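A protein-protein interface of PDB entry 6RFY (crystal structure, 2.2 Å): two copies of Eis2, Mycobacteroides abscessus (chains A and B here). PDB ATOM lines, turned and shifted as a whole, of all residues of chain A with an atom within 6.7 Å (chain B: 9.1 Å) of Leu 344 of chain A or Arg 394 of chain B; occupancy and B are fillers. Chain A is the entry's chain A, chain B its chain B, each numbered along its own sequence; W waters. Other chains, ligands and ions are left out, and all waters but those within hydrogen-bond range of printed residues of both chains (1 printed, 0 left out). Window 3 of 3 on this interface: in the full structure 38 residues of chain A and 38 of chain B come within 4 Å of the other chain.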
ATOM      1  N   GLY A  71      -1.450 -19.564  -6.239  1.00  0.00           N
ATOM      2  CA  GLY A  71      -0.173 -20.227  -6.378  1.00  0.00           C
ATOM      3  C   GLY A  71      -0.153 -21.640  -5.838  1.00  0.00           C
ATOM      4  O   GLY A  71       0.771 -22.399  -6.161  1.00  0.00           O
ATOM      5  N   ARG A 315       1.369 -16.320  -4.019  1.00  0.00           N
ATOM      6  CA  ARG A 315       2.124 -16.001  -5.220  1.00  0.00           C
ATOM      7  C   ARG A 315       1.370 -14.975  -6.053  1.00  0.00           C
ATOM      8  O   ARG A 315       0.182 -14.721  -5.841  1.00  0.00           O
ATOM      9  CB  ARG A 315       2.409 -17.265  -6.038  1.00  0.00           C
ATOM     10  CG  ARG A 315       3.426 -18.161  -5.367  1.00  0.00           C
ATOM     11  CD  ARG A 315       4.696 -17.372  -5.113  1.00  0.00           C
ATOM     12  NE  ARG A 315       5.693 -18.120  -4.359  1.00  0.00           N
ATOM     13  CZ  ARG A 315       5.849 -18.022  -3.043  1.00  0.00           C
ATOM     14  NH1 ARG A 315       5.073 -17.211  -2.334  1.00  0.00           N
ATOM     15  NH2 ARG A 315       6.782 -18.730  -2.434  1.00  0.00           N
ATOM     16  N   TYR A 316       2.086 -14.365  -6.995  1.00  0.00           N
ATOM     17  CA  TYR A 316       1.579 -13.208  -7.715  1.00  0.00           C
ATOM     18  C   TYR A 316       1.620 -13.453  -9.218  1.00  0.00           C
ATOM     19  O   TYR A 316       2.529 -14.109  -9.736  1.00  0.00           O
ATOM     20  CB  TYR A 316       2.374 -11.952  -7.322  1.00  0.00           C
ATOM     21  CG  TYR A 316       2.205 -11.626  -5.850  1.00  0.00           C
ATOM     22  CD1 TYR A 316       3.032 -12.200  -4.888  1.00  0.00           C
ATOM     23  CD2 TYR A 316       1.187 -10.787  -5.418  1.00  0.00           C
ATOM     24  CE1 TYR A 316       2.863 -11.923  -3.537  1.00  0.00           C
ATOM     25  CE2 TYR A 316       1.009 -10.504  -4.070  1.00  0.00           C
ATOM     26  CZ  TYR A 316       1.850 -11.074  -3.135  1.00  0.00           C
ATOM     27  OH  TYR A 316       1.674 -10.794  -1.798  1.00  0.00           O
ATOM     28  N   ALA A 317       0.616 -12.905  -9.913  1.00  0.00           N
ATOM     29  CA  ALA A 317       0.424 -13.209 -11.329  1.00  0.00           C
ATOM     30  C   ALA A 317       1.546 -12.656 -12.192  1.00  0.00           C
ATOM     31  O   ALA A 317       1.797 -13.176 -13.286  1.00  0.00           O
ATOM     32  CB  ALA A 317      -0.924 -12.663 -11.805  1.00  0.00           C
ATOM     33  N   ALA A 318       2.217 -11.603 -11.733  1.00  0.00           N
ATOM     34  CA  ALA A 318       3.353 -11.041 -12.445  1.00  0.00           C
ATOM     35  C   ALA A 318       4.293 -10.404 -11.433  1.00  0.00           C
ATOM     36  O   ALA A 318       3.958 -10.255 -10.254  1.00  0.00           O
ATOM     37  CB  ALA A 318       2.906 -10.025 -13.500  1.00  0.00           C
ATOM     38  N   ASP A 319       5.482 -10.032 -11.904  1.00  0.00           N
ATOM     39  CA  ASP A 319       6.467  -9.421 -11.022  1.00  0.00           C
ATOM     40  C   ASP A 319       5.929  -8.117 -10.447  1.00  0.00           C
ATOM     41  O   ASP A 319       5.242  -7.353 -11.130  1.00  0.00           O
ATOM     42  CB  ASP A 319       7.776  -9.161 -11.773  1.00  0.00           C
ATOM     43  CG  ASP A 319       8.481 -10.442 -12.185  1.00  0.00           C
ATOM     44  OD1 ASP A 319       8.503 -11.395 -11.376  1.00  0.00           O
ATOM     45  OD2 ASP A 319       9.015 -10.497 -13.314  1.00  0.00           O
ATOM     46  N   GLY A 342       7.415  -9.739  -5.273  1.00  0.00           N
ATOM     47  CA  GLY A 342       6.754 -10.993  -5.574  1.00  0.00           C
ATOM     48  C   GLY A 342       6.716 -11.293  -7.054  1.00  0.00           C
ATOM     49  O   GLY A 342       6.928 -10.420  -7.902  1.00  0.00           O
ATOM     50  N   GLY A 343       6.430 -12.550  -7.345  1.00  0.00           N
ATOM     51  CA  GLY A 343       6.306 -13.034  -8.697  1.00  0.00           C
ATOM     52  C   GLY A 343       5.608 -14.371  -8.686  1.00  0.00           C
ATOM     53  O   GLY A 343       4.929 -14.726  -7.722  1.00  0.00           O
ATOM     54  N   LEU A 344       5.787 -15.126  -9.772  1.00  0.00           N
ATOM     55  CA  LEU A 344       5.145 -16.434  -9.862  1.00  0.00           C
ATOM     56  C   LEU A 344       5.774 -17.446  -8.905  1.00  0.00           C
ATOM     57  O   LEU A 344       5.064 -18.273  -8.322  1.00  0.00           O
ATOM     58  CB  LEU A 344       5.186 -16.944 -11.303  1.00  0.00           C
ATOM     59  CG  LEU A 344       4.106 -16.345 -12.212  1.00  0.00           C
ATOM     60  CD1 LEU A 344       4.280 -16.782 -13.658  1.00  0.00           C
ATOM     61  CD2 LEU A 344       2.722 -16.717 -11.706  1.00  0.00           C
ATOM     62  N   ASP A 345       7.096 -17.394  -8.713  1.00  0.00           N
ATOM     63  CA  ASP A 345       7.783 -18.410  -7.925  1.00  0.00           C
ATOM     64  C   ASP A 345       8.436 -17.878  -6.656  1.00  0.00           C
ATOM     65  O   ASP A 345       9.121 -18.644  -5.968  1.00  0.00           O
ATOM     66  CB  ASP A 345       8.852 -19.121  -8.770  1.00  0.00           C
ATOM     67  CG  ASP A 345       9.916 -18.176  -9.290  1.00  0.00           C
ATOM     68  OD1 ASP A 345       9.735 -16.944  -9.183  1.00  0.00           O
ATOM     69  OD2 ASP A 345      10.944 -18.668  -9.802  1.00  0.00           O
ATOM     70  N   HIS A 346       8.260 -16.601  -6.327  1.00  0.00           N
ATOM     71  CA  HIS A 346       8.905 -16.042  -5.149  1.00  0.00           C
ATOM     72  C   HIS A 346       8.009 -14.963  -4.560  1.00  0.00           C
ATOM     73  O   HIS A 346       7.173 -14.378  -5.253  1.00  0.00           O
ATOM     74  CB  HIS A 346      10.285 -15.459  -5.481  1.00  0.00           C
ATOM     75  CG  HIS A 346      10.224 -14.155  -6.215  1.00  0.00           C
ATOM     76  ND1 HIS A 346      10.044 -14.075  -7.579  1.00  0.00           N
ATOM     77  CD2 HIS A 346      10.288 -12.879  -5.768  1.00  0.00           C
ATOM     78  CE1 HIS A 346      10.013 -12.805  -7.943  1.00  0.00           C
ATOM     79  NE2 HIS A 346      10.159 -12.059  -6.864  1.00  0.00           N
ATOM     80  N   TRP A 401      -5.140 -12.878 -10.345  1.00  0.00           N
ATOM     81  CA  TRP A 401      -4.802 -14.273 -10.592  1.00  0.00           C
ATOM     82  C   TRP A 401      -5.621 -14.771 -11.768  1.00  0.00           C
ATOM     83  O   TRP A 401      -6.781 -14.361 -11.911  1.00  0.00           O
ATOM     84  CB  TRP A 401      -5.072 -15.134  -9.352  1.00  0.00           C
ATOM     85  CG  TRP A 401      -4.377 -16.460  -9.372  1.00  0.00           C
ATOM     86  CD1 TRP A 401      -4.960 -17.693  -9.450  1.00  0.00           C
ATOM     87  CD2 TRP A 401      -2.964 -16.688  -9.313  1.00  0.00           C
ATOM     88  NE1 TRP A 401      -3.997 -18.673  -9.444  1.00  0.00           N
ATOM     89  CE2 TRP A 401      -2.763 -18.082  -9.362  1.00  0.00           C
ATOM     90  CE3 TRP A 401      -1.848 -15.848  -9.224  1.00  0.00           C
ATOM     91  CZ2 TRP A 401      -1.492 -18.655  -9.325  1.00  0.00           C
ATOM     92  CZ3 TRP A 401      -0.586 -16.420  -9.187  1.00  0.00           C
ATOM     93  CH2 TRP A 401      -0.419 -17.810  -9.237  1.00  0.00           C
ATOM     94  N   PRO A 402      -5.066 -15.628 -12.630  1.00  0.00           N
ATOM     95  CA  PRO A 402      -5.842 -16.117 -13.781  1.00  0.00           C
ATOM     96  C   PRO A 402      -7.053 -16.946 -13.390  1.00  0.00           C
ATOM     97  O   PRO A 402      -7.996 -17.055 -14.185  1.00  0.00           O
ATOM     98  CB  PRO A 402      -4.823 -16.956 -14.565  1.00  0.00           C
ATOM     99  CG  PRO A 402      -3.488 -16.475 -14.102  1.00  0.00           C
ATOM    100  CD  PRO A 402      -3.667 -16.081 -12.672  1.00  0.00           C
ATOM    101  N   TYR B 316      -0.628  -5.130 -22.973  1.00  0.00           N
ATOM    102  CA  TYR B 316      -0.835  -6.305 -22.145  1.00  0.00           C
ATOM    103  C   TYR B 316      -0.445  -6.011 -20.704  1.00  0.00           C
ATOM    104  O   TYR B 316       0.469  -5.225 -20.439  1.00  0.00           O
ATOM    105  CB  TYR B 316      -0.051  -7.495 -22.708  1.00  0.00           C
ATOM    106  CG  TYR B 316      -0.535  -7.878 -24.089  1.00  0.00           C
ATOM    107  CD1 TYR B 316      -0.017  -7.263 -25.222  1.00  0.00           C
ATOM    108  CD2 TYR B 316      -1.538  -8.823 -24.258  1.00  0.00           C
ATOM    109  CE1 TYR B 316      -0.468  -7.595 -26.486  1.00  0.00           C
ATOM    110  CE2 TYR B 316      -1.996  -9.162 -25.519  1.00  0.00           C
ATOM    111  CZ  TYR B 316      -1.458  -8.545 -26.628  1.00  0.00           C
ATOM    112  OH  TYR B 316      -1.914  -8.881 -27.882  1.00  0.00           O
ATOM    113  N   ALA B 317      -1.170  -6.646 -19.773  1.00  0.00           N
ATOM    114  CA  ALA B 317      -1.028  -6.343 -18.352  1.00  0.00           C
ATOM    115  C   ALA B 317       0.339  -6.719 -17.810  1.00  0.00           C
ATOM    116  O   ALA B 317       0.776  -6.144 -16.808  1.00  0.00           O
ATOM    117  CB  ALA B 317      -2.111  -7.062 -17.547  1.00  0.00           C
ATOM    118  N   ALA B 318       1.016  -7.667 -18.446  1.00  0.00           N
ATOM    119  CA  ALA B 318       2.363  -8.047 -18.061  1.00  0.00           C
ATOM    120  C   ALA B 318       3.087  -8.539 -19.303  1.00  0.00           C
ATOM    121  O   ALA B 318       2.485  -8.734 -20.362  1.00  0.00           O
ATOM    122  CB  ALA B 318       2.347  -9.116 -16.966  1.00  0.00           C
ATOM    123  N   ASP B 319       4.399  -8.719 -19.169  1.00  0.00           N
ATOM    124  CA  ASP B 319       5.195  -9.203 -20.287  1.00  0.00           C
ATOM    125  C   ASP B 319       4.729 -10.595 -20.692  1.00  0.00           C
ATOM    126  O   ASP B 319       4.350 -11.411 -19.848  1.00  0.00           O
ATOM    127  CB  ASP B 319       6.680  -9.224 -19.922  1.00  0.00           C
ATOM    128  CG  ASP B 319       7.248  -7.833 -19.706  1.00  0.00           C
ATOM    129  OD1 ASP B 319       6.890  -6.915 -20.475  1.00  0.00           O
ATOM    130  OD2 ASP B 319       8.059  -7.658 -18.773  1.00  0.00           O
ATOM    131  N   VAL B 320       4.752 -10.863 -21.995  1.00  0.00           N
ATOM    132  CA  VAL B 320       4.324 -12.154 -22.522  1.00  0.00           C
ATOM    133  C   VAL B 320       5.135 -12.464 -23.771  1.00  0.00           C
ATOM    134  O   VAL B 320       5.395 -11.583 -24.596  1.00  0.00           O
ATOM    135  CB  VAL B 320       2.807 -12.169 -22.817  1.00  0.00           C
ATOM    136  CG1 VAL B 320       2.420 -11.031 -23.758  1.00  0.00           C
ATOM    137  CG2 VAL B 320       2.368 -13.517 -23.383  1.00  0.00           C
ATOM    138  N   ASP B 321       5.552 -13.724 -23.894  1.00  0.00           N
ATOM    139  CA  ASP B 321       6.217 -14.229 -25.095  1.00  0.00           C
ATOM    140  C   ASP B 321       5.642 -15.621 -25.340  1.00  0.00           C
ATOM    141  O   ASP B 321       6.078 -16.595 -24.718  1.00  0.00           O
ATOM    142  CB  ASP B 321       7.732 -14.263 -24.930  1.00  0.00           C
ATOM    143  CG  ASP B 321       8.464 -14.523 -26.239  1.00  0.00           C
ATOM    144  OD1 ASP B 321       7.798 -14.804 -27.257  1.00  0.00           O
ATOM    145  OD2 ASP B 321       9.713 -14.442 -26.250  1.00  0.00           O
ATOM    146  N   VAL B 322       4.659 -15.709 -26.235  1.00  0.00           N
ATOM    147  CA  VAL B 322       3.897 -16.936 -26.434  1.00  0.00           C
ATOM    148  C   VAL B 322       3.645 -17.129 -27.924  1.00  0.00           C
ATOM    149  O   VAL B 322       3.527 -16.164 -28.686  1.00  0.00           O
ATOM    150  CB  VAL B 322       2.571 -16.915 -25.634  1.00  0.00           C
ATOM    151  CG1 VAL B 322       1.587 -15.909 -26.227  1.00  0.00           C
ATOM    152  CG2 VAL B 322       1.959 -18.307 -25.553  1.00  0.00           C
ATOM    153  N   LEU B 340       3.490 -13.815 -30.289  1.00  0.00           N
ATOM    154  CA  LEU B 340       3.065 -12.580 -29.647  1.00  0.00           C
ATOM    155  C   LEU B 340       4.105 -12.189 -28.608  1.00  0.00           C
ATOM    156  O   LEU B 340       4.392 -12.963 -27.689  1.00  0.00           O
ATOM    157  CB  LEU B 340       1.694 -12.743 -28.989  1.00  0.00           C
ATOM    158  CG  LEU B 340       1.286 -11.598 -28.059  1.00  0.00           C
ATOM    159  CD1 LEU B 340       1.166 -10.291 -28.828  1.00  0.00           C
ATOM    160  CD2 LEU B 340      -0.004 -11.920 -27.327  1.00  0.00           C
ATOM    161  N   GLY B 342       4.568  -8.989 -26.088  1.00  0.00           N
ATOM    162  CA  GLY B 342       3.873  -7.801 -25.636  1.00  0.00           C
ATOM    163  C   GLY B 342       4.145  -7.493 -24.181  1.00  0.00           C
ATOM    164  O   GLY B 342       4.664  -8.320 -23.427  1.00  0.00           O
ATOM    165  N   ASP B 357       2.819 -22.826 -28.369  1.00  0.00           N
ATOM    166  CA  ASP B 357       2.553 -22.987 -26.946  1.00  0.00           C
ATOM    167  C   ASP B 357       1.082 -23.214 -26.640  1.00  0.00           C
ATOM    168  O   ASP B 357       0.760 -23.942 -25.694  1.00  0.00           O
ATOM    169  CB  ASP B 357       3.039 -21.758 -26.168  1.00  0.00           C
ATOM    170  CG  ASP B 357       4.531 -21.520 -26.317  1.00  0.00           C
ATOM    171  OD1 ASP B 357       5.301 -22.499 -26.272  1.00  0.00           O
ATOM    172  OD2 ASP B 357       4.934 -20.349 -26.472  1.00  0.00           O
ATOM    173  N   ILE B 358       0.187 -22.601 -27.412  1.00  0.00           N
ATOM    174  CA  ILE B 358      -1.247 -22.640 -27.159  1.00  0.00           C
ATOM    175  C   ILE B 358      -1.968 -22.828 -28.486  1.00  0.00           C
ATOM    176  O   ILE B 358      -1.630 -22.185 -29.485  1.00  0.00           O
ATOM    177  CB  ILE B 358      -1.733 -21.354 -26.455  1.00  0.00           C
ATOM    178  CG1 ILE B 358      -1.036 -21.173 -25.106  1.00  0.00           C
ATOM    179  CG2 ILE B 358      -3.237 -21.382 -26.263  1.00  0.00           C
ATOM    180  CD1 ILE B 358      -1.361 -19.865 -24.431  1.00  0.00           C
ATOM    181  N   LEU B 375      -8.148 -16.412 -20.326  1.00  0.00           N
ATOM    182  CA  LEU B 375      -7.677 -17.510 -21.161  1.00  0.00           C
ATOM    183  C   LEU B 375      -7.519 -18.799 -20.363  1.00  0.00           C
ATOM    184  O   LEU B 375      -7.709 -19.893 -20.908  1.00  0.00           O
ATOM    185  CB  LEU B 375      -6.349 -17.129 -21.817  1.00  0.00           C
ATOM    186  CG  LEU B 375      -5.751 -18.101 -22.835  1.00  0.00           C
ATOM    187  CD1 LEU B 375      -6.616 -18.204 -24.086  1.00  0.00           C
ATOM    188  CD2 LEU B 375      -4.327 -17.691 -23.186  1.00  0.00           C
ATOM    189  N   GLN B 376      -7.165 -18.692 -19.079  1.00  0.00           N
ATOM    190  CA  GLN B 376      -7.010 -19.881 -18.247  1.00  0.00           C
ATOM    191  C   GLN B 376      -8.333 -20.616 -18.068  1.00  0.00           C
ATOM    192  O   GLN B 376      -8.373 -21.853 -18.074  1.00  0.00           O
ATOM    193  CB  GLN B 376      -6.415 -19.498 -16.891  1.00  0.00           C
ATOM    194  CG  GLN B 376      -6.231 -20.669 -15.946  1.00  0.00           C
ATOM    195  CD  GLN B 376      -5.229 -21.682 -16.468  1.00  0.00           C
ATOM    196  OE1 GLN B 376      -4.018 -21.484 -16.369  1.00  0.00           O
ATOM    197  NE2 GLN B 376      -5.731 -22.774 -17.031  1.00  0.00           N
ATOM    198  N   GLU B 386      -3.458 -26.151 -24.031  1.00  0.00           N
ATOM    199  CA  GLU B 386      -2.080 -25.795 -23.722  1.00  0.00           C
ATOM    200  C   GLU B 386      -1.148 -26.856 -24.291  1.00  0.00           C
ATOM    201  O   GLU B 386      -1.298 -28.046 -23.997  1.00  0.00           O
ATOM    202  CB  GLU B 386      -1.884 -25.658 -22.211  1.00  0.00           C
ATOM    203  CG  GLU B 386      -0.515 -25.139 -21.804  1.00  0.00           C
ATOM    204  CD  GLU B 386      -0.386 -24.952 -20.305  1.00  0.00           C
ATOM    205  OE1 GLU B 386      -0.416 -25.962 -19.569  1.00  0.00           O
ATOM    206  OE2 GLU B 386      -0.259 -23.789 -19.862  1.00  0.00           O
ATOM    207  N   ARG B 388       2.485 -26.361 -24.271  1.00  0.00           N
ATOM    208  CA  ARG B 388       3.705 -26.361 -23.476  1.00  0.00           C
ATOM    209  C   ARG B 388       3.402 -25.770 -22.108  1.00  0.00           C
ATOM    210  O   ARG B 388       2.657 -24.792 -21.997  1.00  0.00           O
ATOM    211  CB  ARG B 388       4.835 -25.585 -24.165  1.00  0.00           C
ATOM    212  CG  ARG B 388       5.356 -26.257 -25.431  1.00  0.00           C
ATOM    213  CD  ARG B 388       6.407 -25.405 -26.118  1.00  0.00           C
ATOM    214  NE  ARG B 388       7.620 -25.299 -25.311  1.00  0.00           N
ATOM    215  CZ  ARG B 388       8.609 -24.445 -25.554  1.00  0.00           C
ATOM    216  NH1 ARG B 388       8.530 -23.614 -26.585  1.00  0.00           N
ATOM    217  NH2 ARG B 388       9.674 -24.418 -24.763  1.00  0.00           N
ATOM    218  N   ALA B 389       3.995 -26.366 -21.075  1.00  0.00           N
ATOM    219  CA  ALA B 389       3.609 -26.077 -19.699  1.00  0.00           C
ATOM    220  C   ALA B 389       3.853 -24.617 -19.334  1.00  0.00           C
ATOM    221  O   ALA B 389       4.853 -24.014 -19.733  1.00  0.00           O
ATOM    222  CB  ALA B 389       4.375 -26.988 -18.740  1.00  0.00           C
ATOM    223  N   GLY B 390       2.921 -24.052 -18.564  1.00  0.00           N
ATOM    224  CA  GLY B 390       3.038 -22.701 -18.057  1.00  0.00           C
ATOM    225  C   GLY B 390       2.649 -21.602 -19.021  1.00  0.00           C
ATOM    226  O   GLY B 390       2.558 -20.440 -18.602  1.00  0.00           O
ATOM    227  N   ALA B 391       2.409 -21.922 -20.293  1.00  0.00           N
ATOM    228  CA  ALA B 391       2.146 -20.879 -21.280  1.00  0.00           C
ATOM    229  C   ALA B 391       0.806 -20.195 -21.032  1.00  0.00           C
ATOM    230  O   ALA B 391       0.710 -18.964 -21.083  1.00  0.00           O
ATOM    231  CB  ALA B 391       2.194 -21.470 -22.688  1.00  0.00           C
ATOM    232  N   VAL B 392      -0.243 -20.977 -20.765  1.00  0.00           N
ATOM    233  CA  VAL B 392      -1.581 -20.402 -20.641  1.00  0.00           C
ATOM    234  C   VAL B 392      -1.648 -19.429 -19.470  1.00  0.00           C
ATOM    235  O   VAL B 392      -2.223 -18.340 -19.583  1.00  0.00           O
ATOM    236  CB  VAL B 392      -2.635 -21.519 -20.519  1.00  0.00           C
ATOM    237  CG1 VAL B 392      -3.964 -20.953 -20.045  1.00  0.00           C
ATOM    238  CG2 VAL B 392      -2.809 -22.216 -21.855  1.00  0.00           C
ATOM    239  N   GLN B 393      -1.047 -19.793 -18.334  1.00  0.00           N
ATOM    240  CA  GLN B 393      -1.130 -18.937 -17.155  1.00  0.00           C
ATOM    241  C   GLN B 393      -0.463 -17.590 -17.405  1.00  0.00           C
ATOM    242  O   GLN B 393      -1.010 -16.539 -17.051  1.00  0.00           O
ATOM    243  CB  GLN B 393      -0.506 -19.631 -15.946  1.00  0.00           C
ATOM    244  CG  GLN B 393      -1.124 -19.169 -14.641  1.00  0.00           C
ATOM    245  CD  GLN B 393      -0.146 -19.160 -13.490  1.00  0.00           C
ATOM    246  OE1 GLN B 393       0.968 -19.671 -13.600  1.00  0.00           O
ATOM    247  NE2 GLN B 393      -0.557 -18.568 -12.376  1.00  0.00           N
ATOM    248  N   ARG B 394       0.730 -17.602 -18.005  1.00  0.00           N
ATOM    249  CA  ARG B 394       1.397 -16.342 -18.319  1.00  0.00           C
ATOM    250  C   ARG B 394       0.623 -15.560 -19.370  1.00  0.00           C
ATOM    251  O   ARG B 394       0.478 -14.337 -19.257  1.00  0.00           O
ATOM    252  CB  ARG B 394       2.828 -16.594 -18.791  1.00  0.00           C
ATOM    253  CG  ARG B 394       3.846 -16.728 -17.675  1.00  0.00           C
ATOM    254  CD  ARG B 394       5.066 -17.493 -18.154  1.00  0.00           C
ATOM    255  NE  ARG B 394       6.061 -17.662 -17.099  1.00  0.00           N
ATOM    256  CZ  ARG B 394       6.025 -18.624 -16.182  1.00  0.00           C
ATOM    257  NH1 ARG B 394       5.036 -19.507 -16.185  1.00  0.00           N
ATOM    258  NH2 ARG B 394       6.978 -18.700 -15.262  1.00  0.00           N
ATOM    259  N   ALA B 395       0.116 -16.248 -20.396  1.00  0.00           N
ATOM    260  CA  ALA B 395      -0.638 -15.565 -21.442  1.00  0.00           C
ATOM    261  C   ALA B 395      -1.979 -15.056 -20.922  1.00  0.00           C
ATOM    262  O   ALA B 395      -2.447 -13.991 -21.340  1.00  0.00           O
ATOM    263  CB  ALA B 395      -0.839 -16.496 -22.636  1.00  0.00           C
ATOM    264  N   ALA B 396      -2.613 -15.800 -20.014  1.00  0.00           N
ATOM    265  CA  ALA B 396      -3.898 -15.363 -19.473  1.00  0.00           C
ATOM    266  C   ALA B 396      -3.743 -14.071 -18.684  1.00  0.00           C
ATOM    267  O   ALA B 396      -4.537 -13.135 -18.836  1.00  0.00           O
ATOM    268  CB  ALA B 396      -4.510 -16.458 -18.598  1.00  0.00           C
ATOM    269  N   THR B 397      -2.723 -14.011 -17.824  1.00  0.00           N
ATOM    270  CA  THR B 397      -2.453 -12.793 -17.070  1.00  0.00           C
ATOM    271  C   THR B 397      -2.193 -11.620 -18.007  1.00  0.00           C
ATOM    272  O   THR B 397      -2.722 -10.521 -17.810  1.00  0.00           O
ATOM    273  CB  THR B 397      -1.259 -13.012 -16.140  1.00  0.00           C
ATOM    274  OG1 THR B 397      -1.590 -13.997 -15.154  1.00  0.00           O
ATOM    275  CG2 THR B 397      -0.882 -11.716 -15.444  1.00  0.00           C
ATOM    276  N   ALA B 398      -1.380 -11.842 -19.043  1.00  0.00           N
ATOM    277  CA  ALA B 398      -1.050 -10.765 -19.970  1.00  0.00           C
ATOM    278  C   ALA B 398      -2.266 -10.321 -20.775  1.00  0.00           C
ATOM    279  O   ALA B 398      -2.433  -9.127 -21.047  1.00  0.00           O
ATOM    280  CB  ALA B 398       0.073 -11.205 -20.902  1.00  0.00           C
ATOM    281  N   PHE B 399      -3.126 -11.265 -21.167  1.00  0.00           N
ATOM    282  CA  PHE B 399      -4.319 -10.913 -21.930  1.00  0.00           C
ATOM    283  C   PHE B 399      -5.371 -10.220 -21.077  1.00  0.00           C
ATOM    284  O   PHE B 399      -6.246  -9.545 -21.628  1.00  0.00           O
ATOM    285  CB  PHE B 399      -4.914 -12.163 -22.576  1.00  0.00           C
ATOM    286  CG  PHE B 399      -4.431 -12.407 -23.978  1.00  0.00           C
ATOM    287  CD1 PHE B 399      -4.922 -11.657 -25.036  1.00  0.00           C
ATOM    288  CD2 PHE B 399      -3.471 -13.373 -24.238  1.00  0.00           C
ATOM    289  CE1 PHE B 399      -4.476 -11.878 -26.329  1.00  0.00           C
ATOM    290  CE2 PHE B 399      -3.020 -13.596 -25.528  1.00  0.00           C
ATOM    291  CZ  PHE B 399      -3.522 -12.847 -26.575  1.00  0.00           C
ATOM    292  N   GLY B 400      -5.299 -10.356 -19.757  1.00  0.00           N
ATOM    293  CA  GLY B 400      -6.176  -9.634 -18.864  1.00  0.00           C
ATOM    294  C   GLY B 400      -5.848  -8.150 -18.829  1.00  0.00           C
ATOM    295  O   GLY B 400      -5.008  -7.637 -19.568  1.00  0.00           O
HETATM  296  O   HOH W   1       0.349 -15.688 -14.510  1.00  0.00           O
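O of Tyr 316 of chain A lies close to N of Leu 344 of chain A (3.4 Å).
O of Gln 393 of chain B sits at hydrogen-bond distance from OG1 of Thr 397 of chain B, 3.2 Å away.
Leu 344 of chain A touches two residues of chain B.
No residue of chain B comes within 4 Å of Gly 343 of chain A.
Printed residues of chain A within 4 Å of Gln 376 of chain B: Pro 402 (3.8 Å).
Of the printed residues of chain A, Ala 318 of chain B touches Ala 318 (3.6 Å).
The nearest residue of chain B that does not touch Leu 344 of chain A is Thr 397 of chain B (6.2 Å).
The nearest printed residue of chain A that does not touch Gln 393 of chain B is Ala 317 of chain A (5.5 Å).
Water W1 lies within hydrogen-bond range of the side-chain hydroxyl of Thr 397 of chain B, the backbone carbonyl oxygen of Gln 393 of chain B and the backbone carbonyl oxygen of Ala 317 of chain A.
OG1 of Thr 397 of chain B touches CB of Ala 317 of chain A, at 3.7 Å.
Ala 318 of chain A touches Ala 318 of chain B.
Gln 393 of chain B touches Leu 344 of chain A.
Arg 394 of chain B touches Leu 344 of chain A.
Trp 401 of chain A touches Gln 393 of chain B.
Pro 402 of chain A touches Gln 376 of chain B (CB to CB, 3.8 Å).
Pro 402 of chain A touches Gln 393 of chain B (CG to CG, 3.6 Å).
CG of Pro 402 of chain A touches OG1 of Thr 397 of chain B, 3.3 Å away.
Of the 13 printed residues of chain A, 5 touch a printed residue of chain B.
Hydrophobic or aromatic side chains of chain A within 4 Å of the printed part of chain B: Ala 317, Ala 318, Leu 344, Trp 401 and Pro 402.
Of the 27 printed residues of chain B, 5 touch a printed residue of chain A.
Printed residues of chain B that touch a printed residue of chain A: Ala 318, Gln 376, Gln 393, Arg 394 and Thr 397.
Hydrophobic or aromatic side chains of chain B within 4 Å of the printed part of chain A: Ala 318.
Among the printed residues, 8 pairs touch across the chains.
Ala 318 of chain A touches its own counterpart, Ala 318 of chain B.
Of the 8 pairs that touch across the chains among the printed residues, 1 has its exchanged pair printed and touching as well.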
